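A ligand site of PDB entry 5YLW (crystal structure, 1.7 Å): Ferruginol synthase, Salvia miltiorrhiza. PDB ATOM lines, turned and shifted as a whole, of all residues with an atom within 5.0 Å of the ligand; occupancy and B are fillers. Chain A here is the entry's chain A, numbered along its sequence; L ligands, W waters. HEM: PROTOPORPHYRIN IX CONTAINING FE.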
ATOM      1  N   ARG A  95     -39.647  -7.230 -12.582  1.00  0.00           N
ATOM      2  CA  ARG A  95     -39.119  -5.924 -12.179  1.00  0.00           C
ATOM      3  C   ARG A  95     -39.927  -4.820 -12.831  1.00  0.00           C
ATOM      4  O   ARG A  95     -40.469  -5.004 -13.924  1.00  0.00           O
ATOM      5  CB  ARG A  95     -37.668  -5.746 -12.684  1.00  0.00           C
ATOM      6  CG  ARG A  95     -36.627  -6.591 -11.937  1.00  0.00           C
ATOM      7  CD  ARG A  95     -35.565  -5.709 -11.278  1.00  0.00           C
ATOM      8  NE  ARG A  95     -34.570  -6.585 -10.647  1.00  0.00           N
ATOM      9  CZ  ARG A  95     -34.604  -6.956  -9.364  1.00  0.00           C
ATOM     10  NH1 ARG A  95     -35.575  -6.514  -8.543  1.00  0.00           N
ATOM     11  NH2 ARG A  95     -33.657  -7.785  -8.914  1.00  0.00           N
ATOM     12  N   MET A 111     -30.207  -9.695 -17.353  1.00  0.00           N
ATOM     13  CA  MET A 111     -30.661 -10.597 -16.275  1.00  0.00           C
ATOM     14  C   MET A 111     -31.291  -9.795 -15.129  1.00  0.00           C
ATOM     15  O   MET A 111     -32.104 -10.313 -14.356  1.00  0.00           O
ATOM     16  CB  MET A 111     -29.448 -11.376 -15.714  1.00  0.00           C
ATOM     17  CG  MET A 111     -29.813 -12.475 -14.727  1.00  0.00           C
ATOM     18  SD  MET A 111     -28.338 -13.241 -14.037  1.00  0.00           S
ATOM     19  CE  MET A 111     -27.742 -11.927 -12.964  1.00  0.00           C
ATOM     20  N   GLY A 112     -30.896  -8.535 -14.994  1.00  0.00           N
ATOM     21  CA  GLY A 112     -31.431  -7.700 -13.907  1.00  0.00           C
ATOM     22  C   GLY A 112     -32.864  -7.239 -14.144  1.00  0.00           C
ATOM     23  O   GLY A 112     -33.520  -6.786 -13.204  1.00  0.00           O
ATOM     24  N   PHE A 113     -33.358  -7.373 -15.382  1.00  0.00           N
ATOM     25  CA  PHE A 113     -34.662  -6.768 -15.737  1.00  0.00           C
ATOM     26  C   PHE A 113     -35.614  -7.648 -16.531  1.00  0.00           C
ATOM     27  O   PHE A 113     -36.820  -7.393 -16.539  1.00  0.00           O
ATOM     28  CB  PHE A 113     -34.458  -5.414 -16.420  1.00  0.00           C
ATOM     29  CG  PHE A 113     -33.714  -4.434 -15.558  1.00  0.00           C
ATOM     30  CD1 PHE A 113     -34.388  -3.641 -14.624  1.00  0.00           C
ATOM     31  CD2 PHE A 113     -32.322  -4.394 -15.593  1.00  0.00           C
ATOM     32  CE1 PHE A 113     -33.674  -2.784 -13.788  1.00  0.00           C
ATOM     33  CE2 PHE A 113     -31.602  -3.555 -14.762  1.00  0.00           C
ATOM     34  CZ  PHE A 113     -32.286  -2.729 -13.843  1.00  0.00           C
ATOM     35  N   TRP A 120     -33.352 -15.459 -18.542  1.00  0.00           N
ATOM     36  CA  TRP A 120     -32.993 -15.108 -17.179  1.00  0.00           C
ATOM     37  C   TRP A 120     -32.478 -16.314 -16.400  1.00  0.00           C
ATOM     38  O   TRP A 120     -31.426 -16.252 -15.745  1.00  0.00           O
ATOM     39  CB  TRP A 120     -34.210 -14.486 -16.500  1.00  0.00           C
ATOM     40  CG  TRP A 120     -34.004 -14.140 -15.048  1.00  0.00           C
ATOM     41  CD1 TRP A 120     -33.512 -12.950 -14.519  1.00  0.00           C
ATOM     42  CD2 TRP A 120     -34.289 -14.993 -13.894  1.00  0.00           C
ATOM     43  NE1 TRP A 120     -33.496 -13.002 -13.146  1.00  0.00           N
ATOM     44  CE2 TRP A 120     -33.938 -14.215 -12.711  1.00  0.00           C
ATOM     45  CE3 TRP A 120     -34.783 -16.300 -13.730  1.00  0.00           C
ATOM     46  CZ2 TRP A 120     -34.081 -14.716 -11.435  1.00  0.00           C
ATOM     47  CZ3 TRP A 120     -34.906 -16.812 -12.425  1.00  0.00           C
ATOM     48  CH2 TRP A 120     -34.566 -16.033 -11.306  1.00  0.00           C
ATOM     49  N   ARG A 124     -28.861 -16.717 -14.640  1.00  0.00           N
ATOM     50  CA  ARG A 124     -28.776 -16.968 -13.195  1.00  0.00           C
ATOM     51  C   ARG A 124     -27.940 -18.229 -12.894  1.00  0.00           C
ATOM     52  O   ARG A 124     -27.157 -18.233 -11.959  1.00  0.00           O
ATOM     53  CB  ARG A 124     -30.154 -17.132 -12.555  1.00  0.00           C
ATOM     54  CG  ARG A 124     -31.045 -15.887 -12.583  1.00  0.00           C
ATOM     55  CD  ARG A 124     -30.661 -14.818 -11.542  1.00  0.00           C
ATOM     56  NE  ARG A 124     -30.676 -15.311 -10.167  1.00  0.00           N
ATOM     57  CZ  ARG A 124     -30.658 -14.535  -9.073  1.00  0.00           C
ATOM     58  NH1 ARG A 124     -30.697 -13.192  -9.208  1.00  0.00           N
ATOM     59  NH2 ARG A 124     -30.620 -15.082  -7.857  1.00  0.00           N
ATOM     60  N   PHE A 132     -19.855 -17.301  -9.578  1.00  0.00           N
ATOM     61  CA  PHE A 132     -19.821 -17.063  -8.132  1.00  0.00           C
ATOM     62  C   PHE A 132     -19.716 -18.346  -7.321  1.00  0.00           C
ATOM     63  O   PHE A 132     -19.990 -18.341  -6.136  1.00  0.00           O
ATOM     64  CB  PHE A 132     -21.049 -16.238  -7.697  1.00  0.00           C
ATOM     65  CG  PHE A 132     -21.091 -14.896  -8.350  1.00  0.00           C
ATOM     66  CD1 PHE A 132     -20.261 -13.860  -7.894  1.00  0.00           C
ATOM     67  CD2 PHE A 132     -21.922 -14.667  -9.445  1.00  0.00           C
ATOM     68  CE1 PHE A 132     -20.267 -12.609  -8.518  1.00  0.00           C
ATOM     69  CE2 PHE A 132     -21.937 -13.418 -10.074  1.00  0.00           C
ATOM     70  CZ  PHE A 132     -21.123 -12.390  -9.605  1.00  0.00           C
ATOM     71  N   MET A 179     -13.299  -5.329  -8.615  1.00  0.00           N
ATOM     72  CA  MET A 179     -14.230  -5.794  -9.638  1.00  0.00           C
ATOM     73  C   MET A 179     -13.518  -6.063 -10.974  1.00  0.00           C
ATOM     74  O   MET A 179     -13.728  -7.115 -11.561  1.00  0.00           O
ATOM     75  CB  MET A 179     -15.398  -4.794  -9.834  1.00  0.00           C
ATOM     76  CG  MET A 179     -16.301  -4.694  -8.596  1.00  0.00           C
ATOM     77  SD  MET A 179     -17.235  -6.187  -8.198  1.00  0.00           S
ATOM     78  CE  MET A 179     -18.241  -6.345  -9.678  1.00  0.00           C
ATOM     79  N   ASP A 294     -23.880  -5.549 -16.054  1.00  0.00           N
ATOM     80  CA  ASP A 294     -24.707  -5.614 -14.831  1.00  0.00           C
ATOM     81  C   ASP A 294     -23.901  -6.022 -13.606  1.00  0.00           C
ATOM     82  O   ASP A 294     -24.101  -5.481 -12.496  1.00  0.00           O
ATOM     83  CB  ASP A 294     -25.866  -6.590 -14.987  1.00  0.00           C
ATOM     84  CG  ASP A 294     -27.003  -6.026 -15.817  1.00  0.00           C
ATOM     85  OD1 ASP A 294     -27.274  -4.811 -15.678  1.00  0.00           O
ATOM     86  OD2 ASP A 294     -27.610  -6.796 -16.603  1.00  0.00           O
ATOM     87  N   LEU A 295     -22.984  -6.972 -13.792  1.00  0.00           N
ATOM     88  CA  LEU A 295     -22.160  -7.409 -12.652  1.00  0.00           C
ATOM     89  C   LEU A 295     -21.246  -6.264 -12.220  1.00  0.00           C
ATOM     90  O   LEU A 295     -21.121  -5.960 -11.023  1.00  0.00           O
ATOM     91  CB  LEU A 295     -21.368  -8.685 -13.000  1.00  0.00           C
ATOM     92  CG  LEU A 295     -22.246  -9.915 -13.342  1.00  0.00           C
ATOM     93  CD1 LEU A 295     -21.393 -11.133 -13.673  1.00  0.00           C
ATOM     94  CD2 LEU A 295     -23.225 -10.282 -12.238  1.00  0.00           C
ATOM     95  N   GLY A 298     -23.415  -3.460 -10.768  1.00  0.00           N
ATOM     96  CA  GLY A 298     -24.047  -4.009  -9.556  1.00  0.00           C
ATOM     97  C   GLY A 298     -23.163  -3.951  -8.325  1.00  0.00           C
ATOM     98  O   GLY A 298     -23.643  -3.636  -7.237  1.00  0.00           O
ATOM     99  N   GLY A 299     -21.887  -4.235  -8.518  1.00  0.00           N
ATOM    100  CA  GLY A 299     -20.919  -4.303  -7.413  1.00  0.00           C
ATOM    101  C   GLY A 299     -20.178  -3.005  -7.098  1.00  0.00           C
ATOM    102  O   GLY A 299     -19.364  -2.975  -6.170  1.00  0.00           O
ATOM    103  N   THR A 302     -22.692  -0.060  -4.595  1.00  0.00           N
ATOM    104  CA  THR A 302     -23.107  -0.805  -3.391  1.00  0.00           C
ATOM    105  C   THR A 302     -21.925  -1.037  -2.446  1.00  0.00           C
ATOM    106  O   THR A 302     -22.007  -0.735  -1.254  1.00  0.00           O
ATOM    107  CB  THR A 302     -23.658  -2.190  -3.765  1.00  0.00           C
ATOM    108  OG1 THR A 302     -22.764  -2.804  -4.701  1.00  0.00           O
ATOM    109  CG2 THR A 302     -25.063  -2.077  -4.369  1.00  0.00           C
ATOM    110  N   ASN A 303     -20.840  -1.573  -2.979  1.00  0.00           N
ATOM    111  CA  ASN A 303     -19.677  -1.865  -2.126  1.00  0.00           C
ATOM    112  C   ASN A 303     -18.952  -0.582  -1.672  1.00  0.00           C
ATOM    113  O   ASN A 303     -18.487  -0.489  -0.534  1.00  0.00           O
ATOM    114  CB  ASN A 303     -18.709  -2.806  -2.847  1.00  0.00           C
ATOM    115  CG  ASN A 303     -19.197  -4.255  -2.852  1.00  0.00           C
ATOM    116  OD1 ASN A 303     -19.504  -4.811  -1.805  1.00  0.00           O
ATOM    117  ND2 ASN A 303     -19.224  -4.882  -4.046  1.00  0.00           N
ATOM    118  N   SER A 306     -20.919   1.039   1.134  1.00  0.00           N
ATOM    119  CA  SER A 306     -20.892   0.173   2.315  1.00  0.00           C
ATOM    120  C   SER A 306     -19.534   0.172   3.069  1.00  0.00           C
ATOM    121  O   SER A 306     -19.505   0.145   4.304  1.00  0.00           O
ATOM    122  CB  SER A 306     -21.316  -1.256   1.937  1.00  0.00           C
ATOM    123  OG  SER A 306     -22.637  -1.252   1.366  1.00  0.00           O
ATOM    124  N   MET A 357     -24.807  -3.658   7.170  1.00  0.00           N
ATOM    125  CA  MET A 357     -25.884  -3.982   6.214  1.00  0.00           C
ATOM    126  C   MET A 357     -27.272  -3.760   6.798  1.00  0.00           C
ATOM    127  O   MET A 357     -28.226  -3.420   6.074  1.00  0.00           O
ATOM    128  CB  MET A 357     -25.792  -5.457   5.736  1.00  0.00           C
ATOM    129  CG  MET A 357     -24.657  -5.756   4.756  1.00  0.00           C
ATOM    130  SD  MET A 357     -24.739  -4.824   3.210  1.00  0.00           S
ATOM    131  CE  MET A 357     -23.887  -3.291   3.597  1.00  0.00           C
ATOM    132  N   PRO A 362     -27.338  -0.432   1.079  1.00  0.00           N
ATOM    133  CA  PRO A 362     -27.001   0.656   0.146  1.00  0.00           C
ATOM    134  C   PRO A 362     -28.175   1.021  -0.755  1.00  0.00           C
ATOM    135  O   PRO A 362     -28.342   2.187  -1.101  1.00  0.00           O
ATOM    136  CB  PRO A 362     -25.817   0.085  -0.658  1.00  0.00           C
ATOM    137  CG  PRO A 362     -25.904  -1.413  -0.491  1.00  0.00           C
ATOM    138  CD  PRO A 362     -26.454  -1.594   0.925  1.00  0.00           C
ATOM    139  N   LEU A 366     -34.248  -1.624  -2.000  1.00  0.00           N
ATOM    140  CA  LEU A 366     -33.723  -2.682  -2.885  1.00  0.00           C
ATOM    141  C   LEU A 366     -33.781  -2.272  -4.373  1.00  0.00           C
ATOM    142  O   LEU A 366     -33.502  -1.104  -4.705  1.00  0.00           O
ATOM    143  CB  LEU A 366     -34.429  -4.038  -2.571  1.00  0.00           C
ATOM    144  CG  LEU A 366     -34.413  -4.412  -1.065  1.00  0.00           C
ATOM    145  CD1 LEU A 366     -34.875  -5.856  -0.868  1.00  0.00           C
ATOM    146  CD2 LEU A 366     -33.026  -4.249  -0.422  1.00  0.00           C
ATOM    147  N   LEU A 367     -34.091  -3.226  -5.253  1.00  0.00           N
ATOM    148  CA  LEU A 367     -34.442  -2.955  -6.642  1.00  0.00           C
ATOM    149  C   LEU A 367     -35.902  -3.316  -6.810  1.00  0.00           C
ATOM    150  O   LEU A 367     -36.383  -4.272  -6.187  1.00  0.00           O
ATOM    151  CB  LEU A 367     -33.590  -3.790  -7.612  1.00  0.00           C
ATOM    152  CG  LEU A 367     -32.090  -3.537  -7.667  1.00  0.00           C
ATOM    153  CD1 LEU A 367     -31.525  -4.332  -8.841  1.00  0.00           C
ATOM    154  CD2 LEU A 367     -31.765  -2.056  -7.797  1.00  0.00           C
ATOM    155  N   ARG A 369     -39.548  -4.680  -7.575  1.00  0.00           N
ATOM    156  CA  ARG A 369     -40.244  -5.846  -8.122  1.00  0.00           C
ATOM    157  C   ARG A 369     -41.543  -5.371  -8.794  1.00  0.00           C
ATOM    158  O   ARG A 369     -41.851  -4.168  -8.794  1.00  0.00           O
ATOM    159  CB  ARG A 369     -40.519  -6.917  -7.035  1.00  0.00           C
ATOM    160  CG  ARG A 369     -39.264  -7.557  -6.412  1.00  0.00           C
ATOM    161  CD  ARG A 369     -38.405  -8.340  -7.453  1.00  0.00           C
ATOM    162  NE  ARG A 369     -37.407  -9.164  -6.719  1.00  0.00           N
ATOM    163  CZ  ARG A 369     -37.666 -10.351  -6.185  1.00  0.00           C
ATOM    164  NH1 ARG A 369     -38.877 -10.897  -6.317  1.00  0.00           N
ATOM    165  NH2 ARG A 369     -36.718 -11.007  -5.505  1.00  0.00           N
ATOM    166  N   LEU A 428     -32.589  -7.863   5.001  1.00  0.00           N
ATOM    167  CA  LEU A 428     -32.780  -8.112   3.570  1.00  0.00           C
ATOM    168  C   LEU A 428     -31.982  -7.162   2.627  1.00  0.00           C
ATOM    169  O   LEU A 428     -32.493  -6.731   1.575  1.00  0.00           O
ATOM    170  CB  LEU A 428     -34.272  -8.049   3.245  1.00  0.00           C
ATOM    171  CG  LEU A 428     -35.109  -9.184   3.863  1.00  0.00           C
ATOM    172  CD1 LEU A 428     -36.566  -8.842   3.545  1.00  0.00           C
ATOM    173  CD2 LEU A 428     -34.672 -10.528   3.260  1.00  0.00           C
ATOM    174  N   PRO A 429     -30.725  -6.854   2.971  1.00  0.00           N
ATOM    175  CA  PRO A 429     -29.989  -5.890   2.157  1.00  0.00           C
ATOM    176  C   PRO A 429     -29.680  -6.386   0.729  1.00  0.00           C
ATOM    177  O   PRO A 429     -29.445  -5.551  -0.139  1.00  0.00           O
ATOM    178  CB  PRO A 429     -28.684  -5.711   2.943  1.00  0.00           C
ATOM    179  CG  PRO A 429     -28.463  -7.089   3.538  1.00  0.00           C
ATOM    180  CD  PRO A 429     -29.855  -7.437   4.018  1.00  0.00           C
ATOM    181  N   PHE A 430     -29.667  -7.709   0.507  1.00  0.00           N
ATOM    182  CA  PHE A 430     -29.467  -8.309  -0.813  1.00  0.00           C
ATOM    183  C   PHE A 430     -30.793  -8.821  -1.398  1.00  0.00           C
ATOM    184  O   PHE A 430     -30.799  -9.560  -2.402  1.00  0.00           O
ATOM    185  CB  PHE A 430     -28.482  -9.493  -0.682  1.00  0.00           C
ATOM    186  CG  PHE A 430     -27.061  -9.104  -0.370  1.00  0.00           C
ATOM    187  CD1 PHE A 430     -26.178  -8.639  -1.376  1.00  0.00           C
ATOM    188  CD2 PHE A 430     -26.559  -9.233   0.947  1.00  0.00           C
ATOM    189  CE1 PHE A 430     -24.848  -8.317  -1.086  1.00  0.00           C
ATOM    190  CE2 PHE A 430     -25.229  -8.910   1.237  1.00  0.00           C
ATOM    191  CZ  PHE A 430     -24.381  -8.435   0.229  1.00  0.00           C
ATOM    192  N   GLY A 431     -31.928  -8.467  -0.795  1.00  0.00           N
ATOM    193  CA  GLY A 431     -33.190  -9.043  -1.244  1.00  0.00           C
ATOM    194  C   GLY A 431     -33.366 -10.512  -0.862  1.00  0.00           C
ATOM    195  O   GLY A 431     -32.710 -11.023   0.041  1.00  0.00           O
ATOM    196  N   SER A 432     -34.272 -11.183  -1.564  1.00  0.00           N
ATOM    197  CA  SER A 432     -34.650 -12.556  -1.230  1.00  0.00           C
ATOM    198  C   SER A 432     -35.553 -13.083  -2.322  1.00  0.00           C
ATOM    199  O   SER A 432     -36.091 -12.311  -3.114  1.00  0.00           O
ATOM    200  CB  SER A 432     -35.422 -12.588   0.114  1.00  0.00           C
ATOM    201  OG  SER A 432     -35.717 -13.930   0.476  1.00  0.00           O
ATOM    202  N   ARG A 435     -35.112 -13.224  -7.258  1.00  0.00           N
ATOM    203  CA  ARG A 435     -34.089 -12.334  -7.810  1.00  0.00           C
ATOM    204  C   ARG A 435     -33.019 -11.903  -6.817  1.00  0.00           C
ATOM    205  O   ARG A 435     -32.312 -10.917  -7.061  1.00  0.00           O
ATOM    206  CB  ARG A 435     -34.689 -11.080  -8.494  1.00  0.00           C
ATOM    207  CG  ARG A 435     -35.889 -11.344  -9.416  1.00  0.00           C
ATOM    208  CD  ARG A 435     -36.221 -10.075 -10.211  1.00  0.00           C
ATOM    209  NE  ARG A 435     -35.347  -9.930 -11.381  1.00  0.00           N
ATOM    210  CZ  ARG A 435     -35.722 -10.080 -12.662  1.00  0.00           C
ATOM    211  NH1 ARG A 435     -36.983 -10.392 -12.997  1.00  0.00           N
ATOM    212  NH2 ARG A 435     -34.816  -9.891 -13.611  1.00  0.00           N
ATOM    213  N   VAL A 436     -32.884 -12.648  -5.725  1.00  0.00           N
ATOM    214  CA  VAL A 436     -31.903 -12.334  -4.678  1.00  0.00           C
ATOM    215  C   VAL A 436     -30.530 -12.067  -5.303  1.00  0.00           C
ATOM    216  O   VAL A 436     -30.153 -12.745  -6.265  1.00  0.00           O
ATOM    217  CB  VAL A 436     -31.851 -13.479  -3.651  1.00  0.00           C
ATOM    218  CG1 VAL A 436     -31.418 -14.804  -4.295  1.00  0.00           C
ATOM    219  CG2 VAL A 436     -30.955 -13.104  -2.469  1.00  0.00           C
ATOM    220  N   CYS A 437     -29.794 -11.098  -4.778  1.00  0.00           N
ATOM    221  CA  CYS A 437     -28.520 -10.685  -5.383  1.00  0.00           C
ATOM    222  C   CYS A 437     -27.607 -11.881  -5.725  1.00  0.00           C
ATOM    223  O   CYS A 437     -27.215 -12.640  -4.821  1.00  0.00           O
ATOM    224  CB  CYS A 437     -27.757  -9.763  -4.429  1.00  0.00           C
ATOM    225  SG  CYS A 437     -26.204  -9.213  -5.188  1.00  0.00           S
ATOM    226  N   PRO A 438     -27.268 -12.045  -7.011  1.00  0.00           N
ATOM    227  CA  PRO A 438     -26.376 -13.159  -7.366  1.00  0.00           C
ATOM    228  C   PRO A 438     -24.907 -12.871  -7.105  1.00  0.00           C
ATOM    229  O   PRO A 438     -24.083 -13.803  -7.129  1.00  0.00           O
ATOM    230  CB  PRO A 438     -26.614 -13.322  -8.868  1.00  0.00           C
ATOM    231  CG  PRO A 438     -26.870 -11.898  -9.333  1.00  0.00           C
ATOM    232  CD  PRO A 438     -27.725 -11.304  -8.211  1.00  0.00           C
ATOM    233  N   GLY A 439     -24.556 -11.605  -6.871  1.00  0.00           N
ATOM    234  CA  GLY A 439     -23.140 -11.216  -6.655  1.00  0.00           C
ATOM    235  C   GLY A 439     -22.713 -11.306  -5.195  1.00  0.00           C
ATOM    236  O   GLY A 439     -21.568 -10.995  -4.881  1.00  0.00           O
ATOM    237  N   LEU A 442     -19.180 -12.469  -4.038  1.00  0.00           N
ATOM    238  CA  LEU A 442     -18.081 -11.529  -4.324  1.00  0.00           C
ATOM    239  C   LEU A 442     -18.232 -10.272  -3.454  1.00  0.00           C
ATOM    240  O   LEU A 442     -17.241  -9.757  -2.935  1.00  0.00           O
ATOM    241  CB  LEU A 442     -18.066 -11.169  -5.821  1.00  0.00           C
ATOM    242  CG  LEU A 442     -16.998 -10.137  -6.274  1.00  0.00           C
ATOM    243  CD1 LEU A 442     -15.586 -10.557  -5.867  1.00  0.00           C
ATOM    244  CD2 LEU A 442     -17.088  -9.976  -7.804  1.00  0.00           C
ATOM    245  N   ALA A 443     -19.463  -9.783  -3.291  1.00  0.00           N
ATOM    246  CA  ALA A 443     -19.665  -8.612  -2.443  1.00  0.00           C
ATOM    247  C   ALA A 443     -19.104  -8.819  -1.035  1.00  0.00           C
ATOM    248  O   ALA A 443     -18.439  -7.941  -0.496  1.00  0.00           O
ATOM    249  CB  ALA A 443     -21.173  -8.256  -2.381  1.00  0.00           C
ATOM    250  N   LEU A 447     -16.321  -6.472   0.789  1.00  0.00           N
ATOM    251  CA  LEU A 447     -16.618  -5.745   2.029  1.00  0.00           C
ATOM    252  C   LEU A 447     -15.722  -6.202   3.173  1.00  0.00           C
ATOM    253  O   LEU A 447     -15.144  -5.358   3.880  1.00  0.00           O
ATOM    254  CB  LEU A 447     -18.069  -5.951   2.419  1.00  0.00           C
ATOM    255  CG  LEU A 447     -19.117  -5.396   1.474  1.00  0.00           C
ATOM    256  CD1 LEU A 447     -20.465  -5.864   2.023  1.00  0.00           C
ATOM    257  CD2 LEU A 447     -19.057  -3.869   1.470  1.00  0.00           C
HETATM  258  CHA HEM L   1     -29.667  -7.610  -7.551  1.00  0.00           C
HETATM  259  CHB HEM L   1     -27.948  -5.700  -3.271  1.00  0.00           C
HETATM  260  CHC HEM L   1     -23.380  -6.345  -4.776  1.00  0.00           C
HETATM  261  CHD HEM L   1     -25.053  -8.015  -9.140  1.00  0.00           C
HETATM  262  C1A HEM L   1     -29.546  -7.080  -6.221  1.00  0.00           C
HETATM  263  C2A HEM L   1     -30.770  -6.751  -5.447  1.00  0.00           C
HETATM  264  C3A HEM L   1     -30.266  -6.183  -4.213  1.00  0.00           C
HETATM  265  C4A HEM L   1     -28.797  -6.196  -4.326  1.00  0.00           C
HETATM  266  CMA HEM L   1     -31.093  -5.682  -3.066  1.00  0.00           C
HETATM  267  CAA HEM L   1     -32.210  -6.977  -5.846  1.00  0.00           C
HETATM  268  CBA HEM L   1     -32.607  -8.326  -5.171  1.00  0.00           C
HETATM  269  CGA HEM L   1     -34.053  -8.717  -5.332  1.00  0.00           C
HETATM  270  O1A HEM L   1     -34.549  -9.520  -4.506  1.00  0.00           O
HETATM  271  O2A HEM L   1     -34.722  -8.235  -6.264  1.00  0.00           O
HETATM  272  C1B HEM L   1     -26.514  -5.713  -3.342  1.00  0.00           C
HETATM  273  C2B HEM L   1     -25.714  -5.204  -2.224  1.00  0.00           C
HETATM  274  C3B HEM L   1     -24.373  -5.415  -2.686  1.00  0.00           C
HETATM  275  C4B HEM L   1     -24.547  -5.973  -4.016  1.00  0.00           C
HETATM  276  CMB HEM L   1     -26.181  -4.682  -0.897  1.00  0.00           C
HETATM  277  CAB HEM L   1     -23.071  -5.084  -2.054  1.00  0.00           C
HETATM  278  CBB HEM L   1     -22.866  -4.950  -0.755  1.00  0.00           C
HETATM  279  C1C HEM L   1     -23.443  -6.960  -6.075  1.00  0.00           C
HETATM  280  C2C HEM L   1     -22.221  -7.464  -6.742  1.00  0.00           C
HETATM  281  C3C HEM L   1     -22.738  -7.951  -8.021  1.00  0.00           C
HETATM  282  C4C HEM L   1     -24.180  -7.705  -8.040  1.00  0.00           C
HETATM  283  CMC HEM L   1     -20.819  -7.498  -6.203  1.00  0.00           C
HETATM  284  CAC HEM L   1     -21.977  -8.579  -9.131  1.00  0.00           C
HETATM  285  CBC HEM L   1     -20.767  -9.069  -8.942  1.00  0.00           C
HETATM  286  C1D HEM L   1     -26.509  -7.992  -9.052  1.00  0.00           C
HETATM  287  C2D HEM L   1     -27.284  -8.397 -10.212  1.00  0.00           C
HETATM  288  C3D HEM L   1     -28.661  -8.277  -9.779  1.00  0.00           C
HETATM  289  C4D HEM L   1     -28.504  -7.826  -8.381  1.00  0.00           C
HETATM  290  CMD HEM L   1     -26.760  -8.765 -11.570  1.00  0.00           C
HETATM  291  CAD HEM L   1     -29.934  -8.558 -10.543  1.00  0.00           C
HETATM  292  CBD HEM L   1     -30.417  -9.962 -10.176  1.00  0.00           C
HETATM  293  CGD HEM L   1     -31.765 -10.310 -10.801  1.00  0.00           C
HETATM  294  O1D HEM L   1     -32.001 -11.501 -11.103  1.00  0.00           O
HETATM  295  O2D HEM L   1     -32.594  -9.396 -11.033  1.00  0.00           O
HETATM  296  NA  HEM L   1     -28.332  -6.630  -5.620  1.00  0.00           N
HETATM  297  NB  HEM L   1     -25.839  -6.130  -4.413  1.00  0.00           N
HETATM  298  NC  HEM L   1     -24.661  -7.027  -6.847  1.00  0.00           N
HETATM  299  ND  HEM L   1     -27.241  -7.653  -7.957  1.00  0.00           N
HETATM  300 FE   HEM L   1     -26.500  -7.080  -6.127  1.00  0.00          FE
HETATM  301  O   HOH W   1     -26.484  -4.957  -7.144  1.00  0.00           O
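An iron atom (FE) of the ligand is bound by the side-chain sulfur of Cys 437, at 2.3 Å.
NH2 of Arg 369 lies within salt-bridge range of O1A of the ligand (2.8 Å).
O2D of the ligand is in salt-bridge range of NE of Arg 435.
O1D of the ligand is in salt-bridge range of NH1 of Arg 124 (2.9 Å).
The guanidinium group (NH2) of Arg 95 lies within salt-bridge range of an oxygen (O2D) of the ligand, 2.9 Å away.
NE1 of Trp 120 lies within hydrogen-bond range of O1D of the ligand, 2.9 Å away.
N of Ser 432 sits at hydrogen-bond distance from O1A of the ligand, 3.4 Å away.
The backbone NH (N) of Cys 437 is in hydrogen-bond range of the backbone carbonyl oxygen (O) of Phe 430 (3.0 Å).
The guanidinium group of Arg 369 lies within hydrogen-bond range of the backbone carbonyl oxygen of Ser 432 (2.8 Å).
The guanidinium group (NH2) of Arg 435 sits close to the backbone carbonyl oxygen (O) of Gly 112 (3.4 Å).
N of Arg 124 sits at hydrogen-bond distance from SD of Met 111 (3.6 Å).
The guanidinium group of Arg 124 is in hydrogen-bond range of the backbone carbonyl oxygen of Val 436 (2.9 Å).
NE of Arg 95 lies within hydrogen-bond range of O of Gly 112, 2.8 Å away.
The indole nitrogen (NE1) of Trp 120 sits close to the backbone carbonyl oxygen (O) of Met 111, at 3.3 Å.
OG1 of Thr 302 sits at hydrogen-bond distance from O of Gly 298 (2.8 Å).
O of Met 111 sits close to O1D of the ligand.
Gly 112 touches the ligand (O to O2D, 3.5 Å).
CZ of Phe 132 touches CBC of the ligand, 3.4 Å away.
Met 179 touches the ligand (CE to CBC, 3.8 Å).
O of Leu 295 touches CAC of the ligand, 3.3 Å away.
Gly 298 touches the ligand.
CA of Gly 299 touches CMC of the ligand (3.4 Å).
Thr 302 touches the ligand.
Asn 303 touches the ligand (OD1 to CBB, 3.5 Å).
Pro 362 touches the ligand.
Leu 366 touches the ligand.
Leu 367 touches the ligand.
O of Pro 429 touches CMA of the ligand, at 3.4 Å.
CE1 of Phe 430 touches C3B of the ligand (3.3 Å).
Gly 431 touches the ligand.
N of Val 436 touches O1A of the ligand, at 3.7 Å.
Pro 438 touches the ligand.
Gly 439 touches the ligand (CA to C3C, 3.6 Å).
Leu 442 touches the ligand.
CB of Ala 443 touches CAB of the ligand (3.7 Å).
Leu 447 touches the ligand (CD1 to CBB, 3.8 Å).
Hydrophobic or aromatic side chains that line the ligand: Met 111, Trp 120, Phe 132, Met 179, Leu 295, Pro 362, Leu 366, Leu 367, Phe 430, Pro 438, Leu 442, Ala 443 and Leu 447.
Within 4 Å of the ligand: Arg 95, Met 111, Gly 112, Trp 120, Arg 124, Phe 132, Met 179, Leu 295, Gly 298, Gly 299, Thr 302, Asn 303, Pro 362, Leu 366, Leu 367, Arg 369, Pro 429, Phe 430, Gly 431, Ser 432, Arg 435, Val 436, Cys 437, Pro 438, Gly 439, Leu 442, Ala 443 and Leu 447.
The nearest printed residue that does not touch the ligand is Asp 294 (4.1 Å).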
